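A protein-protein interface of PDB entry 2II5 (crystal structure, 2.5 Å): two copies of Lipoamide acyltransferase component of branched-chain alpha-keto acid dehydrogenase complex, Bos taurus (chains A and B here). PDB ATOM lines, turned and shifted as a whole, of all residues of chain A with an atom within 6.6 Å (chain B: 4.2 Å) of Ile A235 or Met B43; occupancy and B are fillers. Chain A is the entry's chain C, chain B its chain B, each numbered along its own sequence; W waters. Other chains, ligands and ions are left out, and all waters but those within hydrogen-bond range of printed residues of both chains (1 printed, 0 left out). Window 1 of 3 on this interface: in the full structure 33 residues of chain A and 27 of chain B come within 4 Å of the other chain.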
ATOM      1  N   PHE A  56     -16.446 -15.198  17.843  1.00  0.00           N
ATOM      2  CA  PHE A  56     -16.072 -13.988  17.162  1.00  0.00           C
ATOM      3  C   PHE A  56     -15.598 -13.060  18.252  1.00  0.00           C
ATOM      4  O   PHE A  56     -16.247 -12.979  19.308  1.00  0.00           O
ATOM      5  CB  PHE A  56     -17.331 -13.413  16.469  1.00  0.00           C
ATOM      6  CG  PHE A  56     -17.209 -11.976  16.059  1.00  0.00           C
ATOM      7  CD1 PHE A  56     -16.364 -11.604  15.027  1.00  0.00           C
ATOM      8  CD2 PHE A  56     -17.940 -11.005  16.710  1.00  0.00           C
ATOM      9  CE1 PHE A  56     -16.250 -10.251  14.636  1.00  0.00           C
ATOM     10  CE2 PHE A  56     -17.857  -9.667  16.312  1.00  0.00           C
ATOM     11  CZ  PHE A  56     -17.013  -9.305  15.271  1.00  0.00           C
ATOM     12  N   ILE A 104     -30.733 -11.084  22.896  1.00  0.00           N
ATOM     13  CA  ILE A 104     -30.101 -12.241  22.269  1.00  0.00           C
ATOM     14  C   ILE A 104     -28.729 -12.552  22.895  1.00  0.00           C
ATOM     15  O   ILE A 104     -28.264 -13.678  22.813  1.00  0.00           O
ATOM     16  CB  ILE A 104     -29.998 -12.121  20.715  1.00  0.00           C
ATOM     17  CG1 ILE A 104     -29.851 -13.507  20.080  1.00  0.00           C
ATOM     18  CG2 ILE A 104     -28.883 -11.180  20.273  1.00  0.00           C
ATOM     19  CD1 ILE A 104     -29.884 -13.449  18.535  1.00  0.00           C
ATOM     20  N   LEU A 105     -28.085 -11.576  23.519  1.00  0.00           N
ATOM     21  CA  LEU A 105     -26.789 -11.829  24.162  1.00  0.00           C
ATOM     22  C   LEU A 105     -26.908 -12.553  25.524  1.00  0.00           C
ATOM     23  O   LEU A 105     -25.913 -13.002  26.110  1.00  0.00           O
ATOM     24  CB  LEU A 105     -26.023 -10.527  24.304  1.00  0.00           C
ATOM     25  CG  LEU A 105     -25.389  -9.974  23.053  1.00  0.00           C
ATOM     26  CD1 LEU A 105     -25.067  -8.473  23.183  1.00  0.00           C
ATOM     27  CD2 LEU A 105     -24.117 -10.757  22.760  1.00  0.00           C
ATOM     28  N   ASN A 106     -28.140 -12.687  26.010  1.00  0.00           N
ATOM     29  CA  ASN A 106     -28.391 -13.314  27.304  1.00  0.00           C
ATOM     30  C   ASN A 106     -29.221 -14.542  27.054  1.00  0.00           C
ATOM     31  O   ASN A 106     -30.159 -14.836  27.773  1.00  0.00           O
ATOM     32  CB  ASN A 106     -29.146 -12.321  28.180  1.00  0.00           C
ATOM     33  CG  ASN A 106     -29.183 -12.737  29.640  1.00  0.00           C
ATOM     34  OD1 ASN A 106     -28.163 -12.767  30.308  1.00  0.00           O
ATOM     35  ND2 ASN A 106     -30.384 -13.041  30.146  1.00  0.00           N
ATOM     36  N   ALA A 107     -28.895 -15.261  26.003  1.00  0.00           N
ATOM     37  CA  ALA A 107     -29.712 -16.343  25.499  1.00  0.00           C
ATOM     38  C   ALA A 107     -28.865 -17.564  25.522  1.00  0.00           C
ATOM     39  O   ALA A 107     -27.676 -17.491  25.747  1.00  0.00           O
ATOM     40  CB  ALA A 107     -30.109 -16.048  24.052  1.00  0.00           C
ATOM     41  N   VAL A 198     -23.958 -17.561  25.431  1.00  0.00           N
ATOM     42  CA  VAL A 198     -23.444 -17.085  24.089  1.00  0.00           C
ATOM     43  C   VAL A 198     -22.406 -15.933  24.018  1.00  0.00           C
ATOM     44  O   VAL A 198     -21.901 -15.568  22.915  1.00  0.00           O
ATOM     45  CB  VAL A 198     -24.598 -16.675  23.182  1.00  0.00           C
ATOM     46  CG1 VAL A 198     -25.385 -17.948  22.801  1.00  0.00           C
ATOM     47  CG2 VAL A 198     -25.544 -15.633  23.881  1.00  0.00           C
ATOM     48  N   ALA A 199     -22.116 -15.313  25.161  1.00  0.00           N
ATOM     49  CA  ALA A 199     -21.157 -14.247  25.198  1.00  0.00           C
ATOM     50  C   ALA A 199     -20.449 -14.204  26.545  1.00  0.00           C
ATOM     51  O   ALA A 199     -20.960 -14.698  27.568  1.00  0.00           O
ATOM     52  CB  ALA A 199     -21.839 -12.917  24.926  1.00  0.00           C
ATOM     53  N   ALA A 230     -18.284 -13.845  21.333  1.00  0.00           N
ATOM     54  CA  ALA A 230     -19.699 -14.152  21.108  1.00  0.00           C
ATOM     55  C   ALA A 230     -19.837 -15.251  20.089  1.00  0.00           C
ATOM     56  O   ALA A 230     -19.004 -15.401  19.155  1.00  0.00           O
ATOM     57  CB  ALA A 230     -20.462 -12.924  20.664  1.00  0.00           C
ATOM     58  N   ASP A 231     -20.864 -16.051  20.314  1.00  0.00           N
ATOM     59  CA  ASP A 231     -21.157 -17.202  19.485  1.00  0.00           C
ATOM     60  C   ASP A 231     -21.660 -16.716  18.138  1.00  0.00           C
ATOM     61  O   ASP A 231     -22.852 -16.426  17.991  1.00  0.00           O
ATOM     62  CB  ASP A 231     -22.200 -18.108  20.172  1.00  0.00           C
ATOM     63  CG  ASP A 231     -22.482 -19.404  19.382  1.00  0.00           C
ATOM     64  OD1 ASP A 231     -22.224 -19.481  18.123  1.00  0.00           O
ATOM     65  OD2 ASP A 231     -22.993 -20.370  20.038  1.00  0.00           O
ATOM     66  N   HIS A 232     -20.771 -16.639  17.155  1.00  0.00           N
ATOM     67  CA  HIS A 232     -21.167 -16.083  15.857  1.00  0.00           C
ATOM     68  C   HIS A 232     -22.216 -16.923  15.072  1.00  0.00           C
ATOM     69  O   HIS A 232     -22.740 -16.446  14.046  1.00  0.00           O
ATOM     70  CB  HIS A 232     -19.960 -15.751  14.977  1.00  0.00           C
ATOM     71  CG  HIS A 232     -20.198 -14.572  14.096  1.00  0.00           C
ATOM     72  ND1 HIS A 232     -21.375 -14.389  13.403  1.00  0.00           N
ATOM     73  CD2 HIS A 232     -19.453 -13.477  13.850  1.00  0.00           C
ATOM     74  CE1 HIS A 232     -21.333 -13.244  12.756  1.00  0.00           C
ATOM     75  NE2 HIS A 232     -20.181 -12.663  13.026  1.00  0.00           N
ATOM     76  N   ARG A 233     -22.565 -18.123  15.555  1.00  0.00           N
ATOM     77  CA  ARG A 233     -23.700 -18.849  14.969  1.00  0.00           C
ATOM     78  C   ARG A 233     -25.067 -18.099  15.040  1.00  0.00           C
ATOM     79  O   ARG A 233     -25.911 -18.237  14.157  1.00  0.00           O
ATOM     80  CB  ARG A 233     -23.836 -20.260  15.571  1.00  0.00           C
ATOM     81  CG  ARG A 233     -22.745 -21.207  15.170  1.00  0.00           C
ATOM     82  CD  ARG A 233     -22.864 -22.497  15.865  1.00  0.00           C
ATOM     83  NE  ARG A 233     -22.871 -22.289  17.307  1.00  0.00           N
ATOM     84  CZ  ARG A 233     -23.093 -23.272  18.191  1.00  0.00           C
ATOM     85  NH1 ARG A 233     -23.297 -24.509  17.770  1.00  0.00           N
ATOM     86  NH2 ARG A 233     -23.128 -23.013  19.483  1.00  0.00           N
ATOM     87  N   ILE A 234     -25.284 -17.330  16.099  1.00  0.00           N
ATOM     88  CA  ILE A 234     -26.531 -16.584  16.288  1.00  0.00           C
ATOM     89  C   ILE A 234     -26.344 -15.118  16.664  1.00  0.00           C
ATOM     90  O   ILE A 234     -27.313 -14.344  16.717  1.00  0.00           O
ATOM     91  CB  ILE A 234     -27.407 -17.267  17.338  1.00  0.00           C
ATOM     92  CG1 ILE A 234     -26.578 -17.666  18.563  1.00  0.00           C
ATOM     93  CG2 ILE A 234     -27.920 -18.551  16.764  1.00  0.00           C
ATOM     94  CD1 ILE A 234     -26.773 -16.798  19.700  1.00  0.00           C
ATOM     95  N   ILE A 235     -25.104 -14.714  16.895  1.00  0.00           N
ATOM     96  CA  ILE A 235     -24.814 -13.340  17.228  1.00  0.00           C
ATOM     97  C   ILE A 235     -23.963 -12.688  16.165  1.00  0.00           C
ATOM     98  O   ILE A 235     -22.811 -13.078  15.980  1.00  0.00           O
ATOM     99  CB  ILE A 235     -24.185 -13.217  18.613  1.00  0.00           C
ATOM    100  CG1 ILE A 235     -25.256 -13.641  19.644  1.00  0.00           C
ATOM    101  CG2 ILE A 235     -23.805 -11.763  18.875  1.00  0.00           C
ATOM    102  CD1 ILE A 235     -24.773 -13.760  20.998  1.00  0.00           C
ATOM    103  N   ASP A 236     -24.522 -11.705  15.457  1.00  0.00           N
ATOM    104  CA  ASP A 236     -23.720 -11.038  14.424  1.00  0.00           C
ATOM    105  C   ASP A 236     -22.812  -9.955  14.981  1.00  0.00           C
ATOM    106  O   ASP A 236     -22.957  -9.587  16.159  1.00  0.00           O
ATOM    107  CB  ASP A 236     -24.587 -10.523  13.255  1.00  0.00           C
ATOM    108  CG  ASP A 236     -25.707  -9.488  13.675  1.00  0.00           C
ATOM    109  OD1 ASP A 236     -25.705  -8.895  14.778  1.00  0.00           O
ATOM    110  OD2 ASP A 236     -26.588  -9.244  12.797  1.00  0.00           O
ATOM    111  N   GLY A 237     -21.933  -9.402  14.136  1.00  0.00           N
ATOM    112  CA  GLY A 237     -20.981  -8.369  14.575  1.00  0.00           C
ATOM    113  C   GLY A 237     -21.603  -7.096  15.096  1.00  0.00           C
ATOM    114  O   GLY A 237     -21.153  -6.538  16.068  1.00  0.00           O
ATOM    115  N   ALA A 238     -22.693  -6.672  14.480  1.00  0.00           N
ATOM    116  CA  ALA A 238     -23.354  -5.418  14.788  1.00  0.00           C
ATOM    117  C   ALA A 238     -24.029  -5.505  16.115  1.00  0.00           C
ATOM    118  O   ALA A 238     -24.069  -4.539  16.852  1.00  0.00           O
ATOM    119  CB  ALA A 238     -24.390  -5.082  13.669  1.00  0.00           C
ATOM    120  N   THR A 239     -24.567  -6.658  16.463  1.00  0.00           N
ATOM    121  CA  THR A 239     -25.189  -6.800  17.773  1.00  0.00           C
ATOM    122  C   THR A 239     -24.133  -6.694  18.875  1.00  0.00           C
ATOM    123  O   THR A 239     -24.311  -5.957  19.828  1.00  0.00           O
ATOM    124  CB  THR A 239     -25.841  -8.155  17.909  1.00  0.00           C
ATOM    125  OG1 THR A 239     -26.780  -8.347  16.854  1.00  0.00           O
ATOM    126  CG2 THR A 239     -26.520  -8.269  19.240  1.00  0.00           C
ATOM    127  N   VAL A 240     -23.028  -7.420  18.768  1.00  0.00           N
ATOM    128  CA  VAL A 240     -22.033  -7.289  19.832  1.00  0.00           C
ATOM    129  C   VAL A 240     -21.465  -5.871  19.859  1.00  0.00           C
ATOM    130  O   VAL A 240     -21.243  -5.316  20.927  1.00  0.00           O
ATOM    131  CB  VAL A 240     -20.933  -8.467  19.923  1.00  0.00           C
ATOM    132  CG1 VAL A 240     -20.656  -9.126  18.628  1.00  0.00           C
ATOM    133  CG2 VAL A 240     -19.612  -7.999  20.534  1.00  0.00           C
ATOM    134  N   HIS B  40     -31.622 -17.177   8.971  1.00  0.00           N
ATOM    135  CA  HIS B  40     -30.708 -17.272  10.104  1.00  0.00           C
ATOM    136  C   HIS B  40     -29.952 -18.617  10.118  1.00  0.00           C
ATOM    137  O   HIS B  40     -28.929 -18.750  10.786  1.00  0.00           O
ATOM    138  CB  HIS B  40     -31.422 -16.952  11.436  1.00  0.00           C
ATOM    139  CG  HIS B  40     -32.047 -15.578  11.470  1.00  0.00           C
ATOM    140  ND1 HIS B  40     -33.393 -15.370  11.724  1.00  0.00           N
ATOM    141  CD2 HIS B  40     -31.517 -14.348  11.233  1.00  0.00           C
ATOM    142  CE1 HIS B  40     -33.658 -14.076  11.655  1.00  0.00           C
ATOM    143  NE2 HIS B  40     -32.541 -13.436  11.350  1.00  0.00           N
ATOM    144  N   LYS B  41     -30.444 -19.579   9.332  1.00  0.00           N
ATOM    145  CA  LYS B  41     -29.827 -20.881   9.186  1.00  0.00           C
ATOM    146  C   LYS B  41     -28.456 -20.829   8.499  1.00  0.00           C
ATOM    147  O   LYS B  41     -27.564 -21.610   8.824  1.00  0.00           O
ATOM    148  CB  LYS B  41     -30.754 -21.817   8.404  1.00  0.00           C
ATOM    149  CG  LYS B  41     -31.723 -22.611   9.254  1.00  0.00           C
ATOM    150  CD  LYS B  41     -32.175 -23.831   8.459  1.00  0.00           C
ATOM    151  CE  LYS B  41     -32.199 -25.108   9.312  1.00  0.00           C
ATOM    152  NZ  LYS B  41     -33.615 -25.555   9.543  1.00  0.00           N
ATOM    153  N   ALA B  42     -28.300 -19.946   7.524  1.00  0.00           N
ATOM    154  CA  ALA B  42     -27.027 -19.831   6.818  1.00  0.00           C
ATOM    155  C   ALA B  42     -25.842 -19.473   7.748  1.00  0.00           C
ATOM    156  O   ALA B  42     -24.740 -20.024   7.585  1.00  0.00           O
ATOM    157  CB  ALA B  42     -27.127 -18.835   5.696  1.00  0.00           C
ATOM    158  N   MET B  43     -26.064 -18.556   8.703  1.00  0.00           N
ATOM    159  CA  MET B  43     -25.002 -18.135   9.598  1.00  0.00           C
ATOM    160  C   MET B  43     -24.491 -19.292  10.458  1.00  0.00           C
ATOM    161  O   MET B  43     -23.270 -19.543  10.495  1.00  0.00           O
ATOM    162  CB  MET B  43     -25.415 -16.943  10.459  1.00  0.00           C
ATOM    163  CG  MET B  43     -24.241 -16.032  10.707  1.00  0.00           C
ATOM    164  SD  MET B  43     -24.489 -14.497  11.616  1.00  0.00           S
ATOM    165  CE  MET B  43     -25.500 -14.837  13.077  1.00  0.00           C
ATOM    166  N   VAL B  44     -25.415 -19.994  11.137  1.00  0.00           N
ATOM    167  CA  VAL B  44     -25.103 -21.223  11.843  1.00  0.00           C
ATOM    168  C   VAL B  44     -24.135 -22.103  11.013  1.00  0.00           C
ATOM    169  O   VAL B  44     -23.103 -22.577  11.527  1.00  0.00           O
ATOM    170  CB  VAL B  44     -26.376 -22.020  12.152  1.00  0.00           C
ATOM    171  CG1 VAL B  44     -26.072 -23.241  13.078  1.00  0.00           C
ATOM    172  CG2 VAL B  44     -27.412 -21.126  12.794  1.00  0.00           C
ATOM    173  N   LYS B  45     -24.461 -22.288   9.731  1.00  0.00           N
ATOM    174  CA  LYS B  45     -23.761 -23.263   8.911  1.00  0.00           C
ATOM    175  C   LYS B  45     -22.396 -22.694   8.479  1.00  0.00           C
ATOM    176  O   LYS B  45     -21.363 -23.376   8.592  1.00  0.00           O
ATOM    177  CB  LYS B  45     -24.681 -23.840   7.798  1.00  0.00           C
ATOM    178  CG  LYS B  45     -23.969 -24.349   6.497  1.00  0.00           C
ATOM    179  CD  LYS B  45     -24.882 -25.272   5.512  1.00  0.00           C
ATOM    180  CE  LYS B  45     -26.209 -24.603   4.948  1.00  0.00           C
ATOM    181  NZ  LYS B  45     -26.179 -23.929   3.551  1.00  0.00           N
ATOM    182  N   THR B  46     -22.372 -21.417   8.112  1.00  0.00           N
ATOM    183  CA  THR B  46     -21.134 -20.749   7.749  1.00  0.00           C
ATOM    184  C   THR B  46     -20.177 -20.729   8.963  1.00  0.00           C
ATOM    185  O   THR B  46     -18.975 -21.051   8.850  1.00  0.00           O
ATOM    186  CB  THR B  46     -21.406 -19.316   7.293  1.00  0.00           C
ATOM    187  OG1 THR B  46     -21.973 -19.322   5.994  1.00  0.00           O
ATOM    188  CG2 THR B  46     -20.152 -18.555   7.182  1.00  0.00           C
ATOM    189  N   MET B  47     -20.690 -20.342  10.121  1.00  0.00           N
ATOM    190  CA  MET B  47     -19.795 -20.178  11.223  1.00  0.00           C
ATOM    191  C   MET B  47     -19.303 -21.522  11.779  1.00  0.00           C
ATOM    192  O   MET B  47     -18.126 -21.621  12.132  1.00  0.00           O
ATOM    193  CB  MET B  47     -20.390 -19.273  12.277  1.00  0.00           C
ATOM    194  CG  MET B  47     -20.611 -17.840  11.740  1.00  0.00           C
ATOM    195  SD  MET B  47     -19.085 -16.943  11.438  1.00  0.00           S
ATOM    196  CE  MET B  47     -19.525 -15.921  10.023  1.00  0.00           C
ATOM    197  N   LEU B 134     -26.246 -11.988   8.576  1.00  0.00           N
ATOM    198  CA  LEU B 134     -24.967 -11.779   7.911  1.00  0.00           C
ATOM    199  C   LEU B 134     -25.015 -12.007   6.421  1.00  0.00           C
ATOM    200  O   LEU B 134     -25.298 -13.107   5.923  1.00  0.00           O
ATOM    201  CB  LEU B 134     -23.859 -12.673   8.502  1.00  0.00           C
ATOM    202  CG  LEU B 134     -22.548 -12.504   7.744  1.00  0.00           C
ATOM    203  CD1 LEU B 134     -21.807 -11.171   8.134  1.00  0.00           C
ATOM    204  CD2 LEU B 134     -21.667 -13.730   7.859  1.00  0.00           C
HETATM  205  O   HOH W   1     -28.121 -17.324  13.177  1.00  0.00           O
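SD of Met B43 lies close to ND1 of His A232.
The guanidinium group of Arg A233 is in salt-bridge range of the side-chain carboxylate of Asp A231 (2.7 Å). A ring nitrogen (ND1) of His A232 sits at hydrogen-bond distance from the backbone carbonyl oxygen (O) of Ile A235, at 3.2 Å.
Among the printed residues, merely in contact across the chains: His A232 with Met B47 (3.4 Å), Arg A233 with Met B43 (3.6 Å), Arg A233 with Val B44 (3.5 Å), Ile A234 with Met B43 (3.7 Å) and Ile A235 with Met B43 (3.8 Å).
Ile A235 touches just one residue of chain B: Met B43 (3.8 Å). Printed residues of chain A within 4 Å of Met B43: His A232 (3.3 Å), Arg A233 (3.6 Å), Ile A234 (3.7 Å) and Ile A235 (3.8 Å). Printed residues of chain B within 4 Å of Arg A233: Met B43 (3.6 Å) and Val B44 (3.5 Å). Of the printed residues of chain A, Met B47 touches His A232 (3.4 Å). The nearest printed residue of chain B that does not touch Ile A235 is Met B47 (6.7 Å). The nearest residue of chain A that does not touch Met B43 is Asp A236 (4.1 Å). The nearest printed residue of chain A that does not touch Met B47 is Arg A233 (4.1 Å).
Of the 18 printed residues of chain A, 4 touch a printed residue of chain B. Printed residues of chain B that touch a printed residue of chain A: Met B43, Val B44 and Met B47. Hydrophobic or aromatic side chains of chain B within 4 Å of the printed part of chain A: Met B43, Val B44 and Met B47. Among the printed residues, 6 pairs touch across the chains. Among the printed residues, no Asp or Glu carboxylate lies within 4 Å of a Lys or Arg side-chain nitrogen of the other chain.
No position is printed for both chains.
Water W1 lies within hydrogen-bond range of O of Arg A233 and O of His B40.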
